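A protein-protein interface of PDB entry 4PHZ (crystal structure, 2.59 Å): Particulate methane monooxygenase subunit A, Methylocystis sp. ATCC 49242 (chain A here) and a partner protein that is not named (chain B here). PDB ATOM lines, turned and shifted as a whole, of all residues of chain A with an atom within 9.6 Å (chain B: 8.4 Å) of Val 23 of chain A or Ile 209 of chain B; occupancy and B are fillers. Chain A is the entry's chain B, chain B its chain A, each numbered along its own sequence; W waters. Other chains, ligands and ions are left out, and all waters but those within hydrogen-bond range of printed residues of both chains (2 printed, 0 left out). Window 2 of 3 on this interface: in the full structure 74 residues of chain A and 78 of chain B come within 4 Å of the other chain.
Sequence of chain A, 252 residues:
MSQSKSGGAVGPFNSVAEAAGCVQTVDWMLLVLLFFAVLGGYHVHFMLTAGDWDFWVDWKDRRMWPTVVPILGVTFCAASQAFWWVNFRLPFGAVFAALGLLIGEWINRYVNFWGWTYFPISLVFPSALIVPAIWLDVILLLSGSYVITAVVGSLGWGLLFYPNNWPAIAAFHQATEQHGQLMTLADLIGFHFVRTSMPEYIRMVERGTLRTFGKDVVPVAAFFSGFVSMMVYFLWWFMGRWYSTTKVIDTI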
ATOM      1  N   VAL A  10      -4.203  38.742  -7.813  1.00  0.00           N
ATOM      2  CA  VAL A  10      -3.785  37.468  -8.430  1.00  0.00           C
ATOM      3  C   VAL A  10      -4.834  36.985  -9.456  1.00  0.00           C
ATOM      4  O   VAL A  10      -5.652  36.096  -9.175  1.00  0.00           O
ATOM      5  CB  VAL A  10      -3.386  36.371  -7.390  1.00  0.00           C
ATOM      6  CG1 VAL A  10      -4.488  36.124  -6.358  1.00  0.00           C
ATOM      7  CG2 VAL A  10      -2.956  35.078  -8.083  1.00  0.00           C
ATOM      8  N   PHE A  13      -8.403  36.577 -10.038  1.00  0.00           N
ATOM      9  CA  PHE A  13      -8.948  37.133  -8.802  1.00  0.00           C
ATOM     10  C   PHE A  13      -8.375  38.519  -8.528  1.00  0.00           C
ATOM     11  O   PHE A  13      -7.171  38.744  -8.661  1.00  0.00           O
ATOM     12  CB  PHE A  13      -8.678  36.218  -7.604  1.00  0.00           C
ATOM     13  CG  PHE A  13      -9.167  34.812  -7.785  1.00  0.00           C
ATOM     14  CD1 PHE A  13     -10.518  34.546  -7.977  1.00  0.00           C
ATOM     15  CD2 PHE A  13      -8.273  33.747  -7.750  1.00  0.00           C
ATOM     16  CE1 PHE A  13     -10.964  33.244  -8.143  1.00  0.00           C
ATOM     17  CE2 PHE A  13      -8.712  32.442  -7.906  1.00  0.00           C
ATOM     18  CZ  PHE A  13     -10.058  32.192  -8.106  1.00  0.00           C
ATOM     19  N   SER A  15      -8.227  40.143  -5.599  1.00  0.00           N
ATOM     20  CA  SER A  15      -7.421  40.162  -4.382  1.00  0.00           C
ATOM     21  C   SER A  15      -6.994  38.768  -3.932  1.00  0.00           C
ATOM     22  O   SER A  15      -7.357  37.763  -4.546  1.00  0.00           O
ATOM     23  CB  SER A  15      -8.171  40.887  -3.259  1.00  0.00           C
ATOM     24  OG  SER A  15      -9.571  40.747  -3.419  1.00  0.00           O
ATOM     25  N   VAL A  16      -6.201  38.729  -2.865  1.00  0.00           N
ATOM     26  CA  VAL A  16      -5.837  37.488  -2.193  1.00  0.00           C
ATOM     27  C   VAL A  16      -7.017  36.972  -1.357  1.00  0.00           C
ATOM     28  O   VAL A  16      -7.200  35.761  -1.197  1.00  0.00           O
ATOM     29  CB  VAL A  16      -4.540  37.671  -1.367  1.00  0.00           C
ATOM     30  CG1 VAL A  16      -4.555  36.877  -0.057  1.00  0.00           C
ATOM     31  CG2 VAL A  16      -3.327  37.331  -2.232  1.00  0.00           C
ATOM     32  N   ALA A  17      -7.827  37.892  -0.845  1.00  0.00           N
ATOM     33  CA  ALA A  17      -9.098  37.519  -0.230  1.00  0.00           C
ATOM     34  C   ALA A  17     -10.016  36.822  -1.245  1.00  0.00           C
ATOM     35  O   ALA A  17     -10.513  35.734  -0.963  1.00  0.00           O
ATOM     36  CB  ALA A  17      -9.790  38.731   0.388  1.00  0.00           C
ATOM     37  N   GLU A  18     -10.215  37.429  -2.422  1.00  0.00           N
ATOM     38  CA  GLU A  18     -11.098  36.849  -3.433  1.00  0.00           C
ATOM     39  C   GLU A  18     -10.630  35.472  -3.922  1.00  0.00           C
ATOM     40  O   GLU A  18     -11.456  34.611  -4.224  1.00  0.00           O
ATOM     41  CB  GLU A  18     -11.306  37.790  -4.614  1.00  0.00           C
ATOM     42  CG  GLU A  18     -12.664  37.587  -5.283  1.00  0.00           C
ATOM     43  CD  GLU A  18     -12.789  38.247  -6.653  1.00  0.00           C
ATOM     44  OE1 GLU A  18     -11.757  38.416  -7.337  1.00  0.00           O
ATOM     45  OE2 GLU A  18     -13.931  38.580  -7.054  1.00  0.00           O
ATOM     46  N   ALA A  19      -9.312  35.266  -3.994  1.00  0.00           N
ATOM     47  CA  ALA A  19      -8.749  33.957  -4.344  1.00  0.00           C
ATOM     48  C   ALA A  19      -9.113  32.949  -3.277  1.00  0.00           C
ATOM     49  O   ALA A  19      -9.834  31.988  -3.562  1.00  0.00           O
ATOM     50  CB  ALA A  19      -7.239  34.020  -4.518  1.00  0.00           C
ATOM     51  N   ALA A  20      -8.642  33.193  -2.049  1.00  0.00           N
ATOM     52  CA  ALA A  20      -8.810  32.252  -0.928  1.00  0.00           C
ATOM     53  C   ALA A  20     -10.270  32.007  -0.580  1.00  0.00           C
ATOM     54  O   ALA A  20     -10.637  30.898  -0.236  1.00  0.00           O
ATOM     55  CB  ALA A  20      -8.024  32.714   0.293  1.00  0.00           C
ATOM     56  N   GLY A  21     -11.099  33.038  -0.709  1.00  0.00           N
ATOM     57  CA  GLY A  21     -12.535  32.933  -0.438  1.00  0.00           C
ATOM     58  C   GLY A  21     -13.265  32.061  -1.445  1.00  0.00           C
ATOM     59  O   GLY A  21     -14.129  31.271  -1.074  1.00  0.00           O
ATOM     60  N   CYS A  22     -12.911  32.208  -2.723  1.00  0.00           N
ATOM     61  CA  CYS A  22     -13.485  31.405  -3.807  1.00  0.00           C
ATOM     62  C   CYS A  22     -13.084  29.923  -3.724  1.00  0.00           C
ATOM     63  O   CYS A  22     -13.934  29.031  -3.807  1.00  0.00           O
ATOM     64  CB  CYS A  22     -13.078  31.986  -5.155  1.00  0.00           C
ATOM     65  SG  CYS A  22     -13.419  30.901  -6.560  1.00  0.00           S
ATOM     66  N   VAL A  23     -11.789  29.672  -3.582  1.00  0.00           N
ATOM     67  CA  VAL A  23     -11.279  28.359  -3.177  1.00  0.00           C
ATOM     68  C   VAL A  23     -12.041  27.746  -1.982  1.00  0.00           C
ATOM     69  O   VAL A  23     -12.394  26.573  -2.008  1.00  0.00           O
ATOM     70  CB  VAL A  23      -9.761  28.432  -2.874  1.00  0.00           C
ATOM     71  CG1 VAL A  23      -9.304  27.286  -1.988  1.00  0.00           C
ATOM     72  CG2 VAL A  23      -8.974  28.448  -4.170  1.00  0.00           C
ATOM     73  N   GLN A  24     -12.312  28.527  -0.944  1.00  0.00           N
ATOM     74  CA  GLN A  24     -12.993  27.963   0.215  1.00  0.00           C
ATOM     75  C   GLN A  24     -14.478  27.649  -0.016  1.00  0.00           C
ATOM     76  O   GLN A  24     -14.999  26.696   0.582  1.00  0.00           O
ATOM     77  CB  GLN A  24     -12.759  28.782   1.502  1.00  0.00           C
ATOM     78  CG  GLN A  24     -12.926  27.981   2.791  1.00  0.00           C
ATOM     79  CD  GLN A  24     -12.534  26.506   2.630  1.00  0.00           C
ATOM     80  OE1 GLN A  24     -11.374  26.182   2.354  1.00  0.00           O
ATOM     81  NE2 GLN A  24     -13.513  25.602   2.794  1.00  0.00           N
ATOM     82  N   THR A  25     -15.166  28.400  -0.873  1.00  0.00           N
ATOM     83  CA  THR A  25     -16.565  28.031  -1.080  1.00  0.00           C
ATOM     84  C   THR A  25     -16.728  26.910  -2.109  1.00  0.00           C
ATOM     85  O   THR A  25     -17.652  26.103  -1.992  1.00  0.00           O
ATOM     86  CB  THR A  25     -17.532  29.213  -1.334  1.00  0.00           C
ATOM     87  OG1 THR A  25     -17.533  29.562  -2.721  1.00  0.00           O
ATOM     88  CG2 THR A  25     -17.180  30.419  -0.478  1.00  0.00           C
ATOM     89  N   VAL A  26     -15.830  26.841  -3.092  1.00  0.00           N
ATOM     90  CA  VAL A  26     -15.898  25.775  -4.099  1.00  0.00           C
ATOM     91  C   VAL A  26     -15.506  24.450  -3.450  1.00  0.00           C
ATOM     92  O   VAL A  26     -16.055  23.408  -3.778  1.00  0.00           O
ATOM     93  CB  VAL A  26     -15.072  26.106  -5.373  1.00  0.00           C
ATOM     94  CG1 VAL A  26     -14.948  24.903  -6.294  1.00  0.00           C
ATOM     95  CG2 VAL A  26     -15.725  27.247  -6.144  1.00  0.00           C
ATOM     96  N   ASP A  27     -14.588  24.497  -2.492  1.00  0.00           N
ATOM     97  CA  ASP A  27     -14.276  23.319  -1.682  1.00  0.00           C
ATOM     98  C   ASP A  27     -15.518  22.733  -1.011  1.00  0.00           C
ATOM     99  O   ASP A  27     -15.735  21.524  -1.074  1.00  0.00           O
ATOM    100  CB  ASP A  27     -13.196  23.630  -0.642  1.00  0.00           C
ATOM    101  CG  ASP A  27     -11.808  23.141  -1.067  1.00  0.00           C
ATOM    102  OD1 ASP A  27     -11.580  22.965  -2.283  1.00  0.00           O
ATOM    103  OD2 ASP A  27     -10.934  22.938  -0.182  1.00  0.00           O
ATOM    104  N   TRP A  28     -16.334  23.584  -0.387  1.00  0.00           N
ATOM    105  CA  TRP A  28     -17.597  23.139   0.215  1.00  0.00           C
ATOM    106  C   TRP A  28     -18.543  22.568  -0.796  1.00  0.00           C
ATOM    107  O   TRP A  28     -19.128  21.515  -0.562  1.00  0.00           O
ATOM    108  CB  TRP A  28     -18.292  24.253   1.017  1.00  0.00           C
ATOM    109  CG  TRP A  28     -17.723  24.415   2.403  1.00  0.00           C
ATOM    110  CD1 TRP A  28     -16.980  25.482   2.890  1.00  0.00           C
ATOM    111  CD2 TRP A  28     -17.790  23.458   3.527  1.00  0.00           C
ATOM    112  NE1 TRP A  28     -16.602  25.264   4.195  1.00  0.00           N
ATOM    113  CE2 TRP A  28     -17.053  24.076   4.639  1.00  0.00           C
ATOM    114  CE3 TRP A  28     -18.373  22.207   3.719  1.00  0.00           C
ATOM    115  CZ2 TRP A  28     -16.917  23.452   5.876  1.00  0.00           C
ATOM    116  CZ3 TRP A  28     -18.228  21.587   4.977  1.00  0.00           C
ATOM    117  CH2 TRP A  28     -17.519  22.199   6.027  1.00  0.00           C
ATOM    118  N   MET A  29     -18.701  23.253  -1.921  1.00  0.00           N
ATOM    119  CA  MET A  29     -19.616  22.812  -2.946  1.00  0.00           C
ATOM    120  C   MET A  29     -19.222  21.465  -3.528  1.00  0.00           C
ATOM    121  O   MET A  29     -20.086  20.679  -3.919  1.00  0.00           O
ATOM    122  CB  MET A  29     -19.695  23.830  -4.065  1.00  0.00           C
ATOM    123  CG  MET A  29     -20.297  25.166  -3.669  1.00  0.00           C
ATOM    124  SD  MET A  29     -19.885  26.349  -4.974  1.00  0.00           S
ATOM    125  CE  MET A  29     -21.248  26.102  -6.130  1.00  0.00           C
ATOM    126  N   LEU A  30     -17.929  21.178  -3.583  1.00  0.00           N
ATOM    127  CA  LEU A  30     -17.498  19.902  -4.172  1.00  0.00           C
ATOM    128  C   LEU A  30     -17.802  18.749  -3.234  1.00  0.00           C
ATOM    129  O   LEU A  30     -18.511  17.819  -3.609  1.00  0.00           O
ATOM    130  CB  LEU A  30     -16.018  19.915  -4.585  1.00  0.00           C
ATOM    131  CG  LEU A  30     -15.617  20.872  -5.723  1.00  0.00           C
ATOM    132  CD1 LEU A  30     -14.108  20.806  -5.945  1.00  0.00           C
ATOM    133  CD2 LEU A  30     -16.415  20.664  -7.015  1.00  0.00           C
ATOM    134  N   LEU A  31     -17.290  18.841  -2.014  1.00  0.00           N
ATOM    135  CA  LEU A  31     -17.626  17.927  -0.929  1.00  0.00           C
ATOM    136  C   LEU A  31     -19.075  17.507  -0.909  1.00  0.00           C
ATOM    137  O   LEU A  31     -19.382  16.323  -0.966  1.00  0.00           O
ATOM    138  CB  LEU A  31     -17.372  18.604   0.405  1.00  0.00           C
ATOM    139  CG  LEU A  31     -17.372  17.601   1.543  1.00  0.00           C
ATOM    140  CD1 LEU A  31     -16.143  16.694   1.443  1.00  0.00           C
ATOM    141  CD2 LEU A  31     -17.443  18.329   2.878  1.00  0.00           C
ATOM    142  N   LEU A  34     -20.466  15.973  -4.253  1.00  0.00           N
ATOM    143  CA  LEU A  34     -19.949  14.613  -4.328  1.00  0.00           C
ATOM    144  C   LEU A  34     -20.468  13.760  -3.195  1.00  0.00           C
ATOM    145  O   LEU A  34     -20.534  12.542  -3.320  1.00  0.00           O
ATOM    146  CB  LEU A  34     -18.433  14.586  -4.239  1.00  0.00           C
ATOM    147  CG  LEU A  34     -17.601  15.065  -5.423  1.00  0.00           C
ATOM    148  CD1 LEU A  34     -16.177  15.328  -4.935  1.00  0.00           C
ATOM    149  CD2 LEU A  34     -17.651  14.094  -6.610  1.00  0.00           C
ATOM    150  N   TRP A  84     -10.923   9.467  -4.292  1.00  0.00           N
ATOM    151  CA  TRP A  84     -10.401  10.443  -3.319  1.00  0.00           C
ATOM    152  C   TRP A  84      -8.961  10.346  -3.137  1.00  0.00           C
ATOM    153  O   TRP A  84      -8.287  11.354  -2.963  1.00  0.00           O
ATOM    154  CB  TRP A  84     -11.054  10.333  -1.957  1.00  0.00           C
ATOM    155  CG  TRP A  84     -12.452  10.871  -1.997  1.00  0.00           C
ATOM    156  CD1 TRP A  84     -13.635  10.148  -2.014  1.00  0.00           C
ATOM    157  CD2 TRP A  84     -12.856  12.273  -2.106  1.00  0.00           C
ATOM    158  NE1 TRP A  84     -14.707  10.984  -2.102  1.00  0.00           N
ATOM    159  CE2 TRP A  84     -14.310  12.274  -2.157  1.00  0.00           C
ATOM    160  CE3 TRP A  84     -12.182  13.482  -2.134  1.00  0.00           C
ATOM    161  CZ2 TRP A  84     -15.044  13.448  -2.235  1.00  0.00           C
ATOM    162  CZ3 TRP A  84     -12.927  14.657  -2.221  1.00  0.00           C
ATOM    163  CH2 TRP A  84     -14.328  14.637  -2.267  1.00  0.00           C
ATOM    164  N   ASN A  87      -6.588  11.008  -6.791  1.00  0.00           N
ATOM    165  CA  ASN A  87      -6.476  12.418  -7.161  1.00  0.00           C
ATOM    166  C   ASN A  87      -6.270  13.459  -6.046  1.00  0.00           C
ATOM    167  O   ASN A  87      -6.047  14.615  -6.338  1.00  0.00           O
ATOM    168  CB  ASN A  87      -7.676  12.841  -7.988  1.00  0.00           C
ATOM    169  CG  ASN A  87      -8.090  11.795  -8.978  1.00  0.00           C
ATOM    170  OD1 ASN A  87      -7.327  11.407  -9.855  1.00  0.00           O
ATOM    171  ND2 ASN A  87      -9.312  11.308  -8.829  1.00  0.00           N
ATOM    172  N   PHE A  88      -6.398  13.090  -4.781  1.00  0.00           N
ATOM    173  CA  PHE A  88      -6.345  14.092  -3.712  1.00  0.00           C
ATOM    174  C   PHE A  88      -5.606  13.566  -2.510  1.00  0.00           C
ATOM    175  O   PHE A  88      -5.517  14.261  -1.511  1.00  0.00           O
ATOM    176  CB  PHE A  88      -7.739  14.513  -3.223  1.00  0.00           C
ATOM    177  CG  PHE A  88      -8.703  14.892  -4.314  1.00  0.00           C
ATOM    178  CD1 PHE A  88      -9.326  13.916  -5.086  1.00  0.00           C
ATOM    179  CD2 PHE A  88      -9.045  16.222  -4.527  1.00  0.00           C
ATOM    180  CE1 PHE A  88     -10.224  14.265  -6.082  1.00  0.00           C
ATOM    181  CE2 PHE A  88      -9.952  16.578  -5.508  1.00  0.00           C
ATOM    182  CZ  PHE A  88     -10.537  15.595  -6.289  1.00  0.00           C
ATOM    183  N   LEU A  90      -6.571  12.181  -0.220  1.00  0.00           N
ATOM    184  CA  LEU A  90      -7.491  12.295   0.922  1.00  0.00           C
ATOM    185  C   LEU A  90      -7.974  10.911   1.378  1.00  0.00           C
ATOM    186  O   LEU A  90      -8.556  10.171   0.568  1.00  0.00           O
ATOM    187  CB  LEU A  90      -8.685  13.183   0.537  1.00  0.00           C
ATOM    188  CG  LEU A  90      -8.400  14.685   0.454  1.00  0.00           C
ATOM    189  CD1 LEU A  90      -9.409  15.421  -0.412  1.00  0.00           C
ATOM    190  CD2 LEU A  90      -8.374  15.278   1.856  1.00  0.00           C
ATOM    191  N   PHE B 203     -11.015  17.087   5.343  1.00  0.00           N
ATOM    192  CA  PHE B 203     -11.502  18.145   4.460  1.00  0.00           C
ATOM    193  C   PHE B 203     -10.919  19.502   4.811  1.00  0.00           C
ATOM    194  O   PHE B 203     -10.731  20.352   3.938  1.00  0.00           O
ATOM    195  CB  PHE B 203     -13.013  18.256   4.522  1.00  0.00           C
ATOM    196  CG  PHE B 203     -13.570  19.412   3.729  1.00  0.00           C
ATOM    197  CD1 PHE B 203     -13.574  19.395   2.330  1.00  0.00           C
ATOM    198  CD2 PHE B 203     -14.109  20.509   4.381  1.00  0.00           C
ATOM    199  CE1 PHE B 203     -14.115  20.453   1.603  1.00  0.00           C
ATOM    200  CE2 PHE B 203     -14.649  21.572   3.659  1.00  0.00           C
ATOM    201  CZ  PHE B 203     -14.660  21.545   2.270  1.00  0.00           C
ATOM    202  N   LYS B 206      -6.593  19.619   4.857  1.00  0.00           N
ATOM    203  CA  LYS B 206      -6.136  19.703   3.458  1.00  0.00           C
ATOM    204  C   LYS B 206      -7.326  20.226   2.670  1.00  0.00           C
ATOM    205  O   LYS B 206      -8.477  20.030   3.081  1.00  0.00           O
ATOM    206  CB  LYS B 206      -5.754  18.324   2.906  1.00  0.00           C
ATOM    207  CG  LYS B 206      -5.268  17.328   3.938  1.00  0.00           C
ATOM    208  CD  LYS B 206      -3.807  17.551   4.250  1.00  0.00           C
ATOM    209  CE  LYS B 206      -3.503  17.203   5.692  1.00  0.00           C
ATOM    210  NZ  LYS B 206      -2.632  16.004   5.762  1.00  0.00           N
ATOM    211  N   GLY B 207      -7.107  20.875   1.537  1.00  0.00           N
ATOM    212  CA  GLY B 207      -8.290  21.288   0.764  1.00  0.00           C
ATOM    213  C   GLY B 207      -8.802  20.179  -0.136  1.00  0.00           C
ATOM    214  O   GLY B 207      -8.198  19.116  -0.222  1.00  0.00           O
ATOM    215  N   ILE B 208      -9.902  20.418  -0.827  1.00  0.00           N
ATOM    216  CA  ILE B 208     -10.192  19.561  -1.967  1.00  0.00           C
ATOM    217  C   ILE B 208      -9.258  20.088  -3.072  1.00  0.00           C
ATOM    218  O   ILE B 208      -8.303  19.402  -3.476  1.00  0.00           O
ATOM    219  CB  ILE B 208     -11.714  19.533  -2.331  1.00  0.00           C
ATOM    220  CG1 ILE B 208     -12.503  18.698  -1.299  1.00  0.00           C
ATOM    221  CG2 ILE B 208     -11.956  19.018  -3.759  1.00  0.00           C
ATOM    222  CD1 ILE B 208     -14.001  18.628  -1.545  1.00  0.00           C
ATOM    223  N   ILE B 209      -9.511  21.340  -3.475  1.00  0.00           N
ATOM    224  CA  ILE B 209      -8.759  22.068  -4.500  1.00  0.00           C
ATOM    225  C   ILE B 209      -7.249  22.105  -4.246  1.00  0.00           C
ATOM    226  O   ILE B 209      -6.456  21.837  -5.157  1.00  0.00           O
ATOM    227  CB  ILE B 209      -9.297  23.503  -4.648  1.00  0.00           C
ATOM    228  CG1 ILE B 209     -10.598  23.488  -5.452  1.00  0.00           C
ATOM    229  CG2 ILE B 209      -8.269  24.375  -5.353  1.00  0.00           C
ATOM    230  CD1 ILE B 209     -11.467  24.714  -5.303  1.00  0.00           C
ATOM    231  N   THR B 210      -6.854  22.423  -3.016  1.00  0.00           N
ATOM    232  CA  THR B 210      -5.440  22.416  -2.653  1.00  0.00           C
ATOM    233  C   THR B 210      -4.816  21.054  -2.951  1.00  0.00           C
ATOM    234  O   THR B 210      -3.807  20.958  -3.668  1.00  0.00           O
ATOM    235  CB  THR B 210      -5.222  22.775  -1.167  1.00  0.00           C
ATOM    236  OG1 THR B 210      -5.647  24.127  -0.946  1.00  0.00           O
ATOM    237  CG2 THR B 210      -3.735  22.644  -0.777  1.00  0.00           C
ATOM    238  N   SER B 211      -5.442  20.009  -2.407  1.00  0.00           N
ATOM    239  CA  SER B 211      -4.924  18.653  -2.506  1.00  0.00           C
ATOM    240  C   SER B 211      -4.876  18.202  -3.946  1.00  0.00           C
ATOM    241  O   SER B 211      -3.939  17.501  -4.320  1.00  0.00           O
ATOM    242  CB  SER B 211      -5.754  17.683  -1.663  1.00  0.00           C
ATOM    243  OG  SER B 211      -5.579  17.935  -0.285  1.00  0.00           O
ATOM    244  N   TYR B 212      -5.871  18.600  -4.742  1.00  0.00           N
ATOM    245  CA  TYR B 212      -5.909  18.209  -6.162  1.00  0.00           C
ATOM    246  C   TYR B 212      -4.664  18.730  -6.850  1.00  0.00           C
ATOM    247  O   TYR B 212      -3.867  17.983  -7.463  1.00  0.00           O
ATOM    248  CB  TYR B 212      -7.117  18.795  -6.882  1.00  0.00           C
ATOM    249  CG  TYR B 212      -7.037  18.573  -8.376  1.00  0.00           C
ATOM    250  CD1 TYR B 212      -7.026  17.275  -8.923  1.00  0.00           C
ATOM    251  CD2 TYR B 212      -6.968  19.641  -9.246  1.00  0.00           C
ATOM    252  CE1 TYR B 212      -6.956  17.061 -10.296  1.00  0.00           C
ATOM    253  CE2 TYR B 212      -6.886  19.441 -10.620  1.00  0.00           C
ATOM    254  CZ  TYR B 212      -6.887  18.154 -11.146  1.00  0.00           C
ATOM    255  OH  TYR B 212      -6.831  17.956 -12.518  1.00  0.00           O
ATOM    256  N   ILE B 213      -4.536  20.048  -6.725  1.00  0.00           N
ATOM    257  CA  ILE B 213      -3.393  20.801  -7.221  1.00  0.00           C
ATOM    258  C   ILE B 213      -2.073  20.173  -6.741  1.00  0.00           C
ATOM    259  O   ILE B 213      -1.235  19.795  -7.560  1.00  0.00           O
ATOM    260  CB  ILE B 213      -3.522  22.307  -6.868  1.00  0.00           C
ATOM    261  CG1 ILE B 213      -4.563  22.948  -7.779  1.00  0.00           C
ATOM    262  CG2 ILE B 213      -2.210  23.020  -7.060  1.00  0.00           C
ATOM    263  CD1 ILE B 213      -4.924  24.367  -7.418  1.00  0.00           C
ATOM    264  N   ARG B 214      -1.901  20.018  -5.435  1.00  0.00           N
ATOM    265  CA  ARG B 214      -0.680  19.379  -4.944  1.00  0.00           C
ATOM    266  C   ARG B 214      -0.371  18.072  -5.674  1.00  0.00           C
ATOM    267  O   ARG B 214       0.699  17.917  -6.276  1.00  0.00           O
ATOM    268  CB  ARG B 214      -0.745  19.138  -3.449  1.00  0.00           C
ATOM    269  CG  ARG B 214      -0.316  20.332  -2.649  1.00  0.00           C
ATOM    270  CD  ARG B 214      -0.205  20.014  -1.180  1.00  0.00           C
ATOM    271  NE  ARG B 214      -0.486  21.235  -0.435  1.00  0.00           N
ATOM    272  CZ  ARG B 214      -0.498  21.344   0.889  1.00  0.00           C
ATOM    273  NH1 ARG B 214      -0.237  20.292   1.659  1.00  0.00           N
ATOM    274  NH2 ARG B 214      -0.772  22.521   1.442  1.00  0.00           N
ATOM    275  N   VAL B 215      -1.330  17.146  -5.637  1.00  0.00           N
ATOM    276  CA  VAL B 215      -1.182  15.836  -6.268  1.00  0.00           C
ATOM    277  C   VAL B 215      -0.882  15.977  -7.756  1.00  0.00           C
ATOM    278  O   VAL B 215       0.071  15.362  -8.255  1.00  0.00           O
ATOM    279  CB  VAL B 215      -2.418  14.936  -6.019  1.00  0.00           C
ATOM    280  CG1 VAL B 215      -2.367  13.694  -6.909  1.00  0.00           C
ATOM    281  CG2 VAL B 215      -2.521  14.579  -4.525  1.00  0.00           C
ATOM    282  N   ALA B 216      -1.663  16.808  -8.443  1.00  0.00           N
ATOM    283  CA  ALA B 216      -1.460  17.034  -9.875  1.00  0.00           C
ATOM    284  C   ALA B 216      -0.073  17.628 -10.209  1.00  0.00           C
ATOM    285  O   ALA B 216       0.528  17.262 -11.216  1.00  0.00           O
ATOM    286  CB  ALA B 216      -2.573  17.903 -10.447  1.00  0.00           C
HETATM  287  O   HOH W   1      -8.391  23.798  -0.874  1.00  0.00           O
HETATM  288  O   HOH W   2      -4.680  15.054  -8.768  1.00  0.00           O
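Water W1 bridges OG1 of Thr 210 of chain B and OD2 of Asp 27 of chain A. Water W2 bridges the backbone carbonyl oxygen of Asn 87 of chain A and the backbone carbonyl oxygen of Tyr 212 of chain B.
OD2 of Asp 27 of chain A sits at hydrogen-bond distance from N of Ile 208 of chain B, at 2.8 Å. The side-chain carboxylate (OD1) of Asp 27 of chain A lies within hydrogen-bond range of the backbone NH (N) of Ile 209 of chain B (2.9 Å).
Hydrophobic or aromatic side chains of chain B within 4 Å of the printed part of chain A: Phe 203, Ile 208, Ile 209, Tyr 212 and Val 215. Among the printed residues, no Asp or Glu carboxylate lies within 4 Å of a Lys or Arg side-chain nitrogen of the other chain.
O of Gly 207 of chain B lies within hydrogen-bond range of OG of Ser 211 of chain B, 2.9 Å away. The indole nitrogen (NE1) of Trp 28 of chain A sits close to the side-chain amide nitrogen (NE2) of Gln 24 of chain A (3.4 Å). The backbone carbonyl oxygen (O) of Trp 84 of chain A lies within hydrogen-bond range of the backbone NH (N) of Leu 90 of chain A, 3.3 Å away.
Ile 209 of chain B touches Val 23 of chain A. Val 26 of chain A touches Ile 209 of chain B. CE1 of Phe 203 of chain B touches O of Asp 27 of chain A, 3.3 Å away. CA of Gly 207 of chain B touches OD2 of Asp 27 of chain A, at 3.3 Å. CD1 of Leu 30 of chain A touches CG2 of Ile 208 of chain B, 3.6 Å away. CD1 of Phe 203 of chain B touches CD1 of Leu 31 of chain A, 3.8 Å away. Leu 31 of chain A touches Ile 208 of chain B. Tyr 212 of chain B touches Asn 87 of chain A (CA to O, 3.6 Å). Phe 88 of chain A touches Ile 208 of chain B (CD2 to O, 3.4 Å). Phe 88 of chain A touches Val 215 of chain B.
Cys 22 of chain A touches none of the printed residues of chain B. Printed residues of chain B within 4 Å of Leu 90 of chain A: Gly 207. Printed residues of chain A within 4 Å of Phe 203 of chain B: Asp 27 (3.3 Å), Trp 28 (3.6 Å) and Leu 31 (3.8 Å). Of the printed residues of chain A, Gly 207 of chain B touches Asp 27 (3.3 Å) and Leu 90 (3.9 Å). Ile 209 of chain B touches three residues of chain A. No residue of chain A comes within 4 Å of Thr 210 of chain B. Printed residues of chain A within 4 Å of Ser 211 of chain B: Phe 88.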
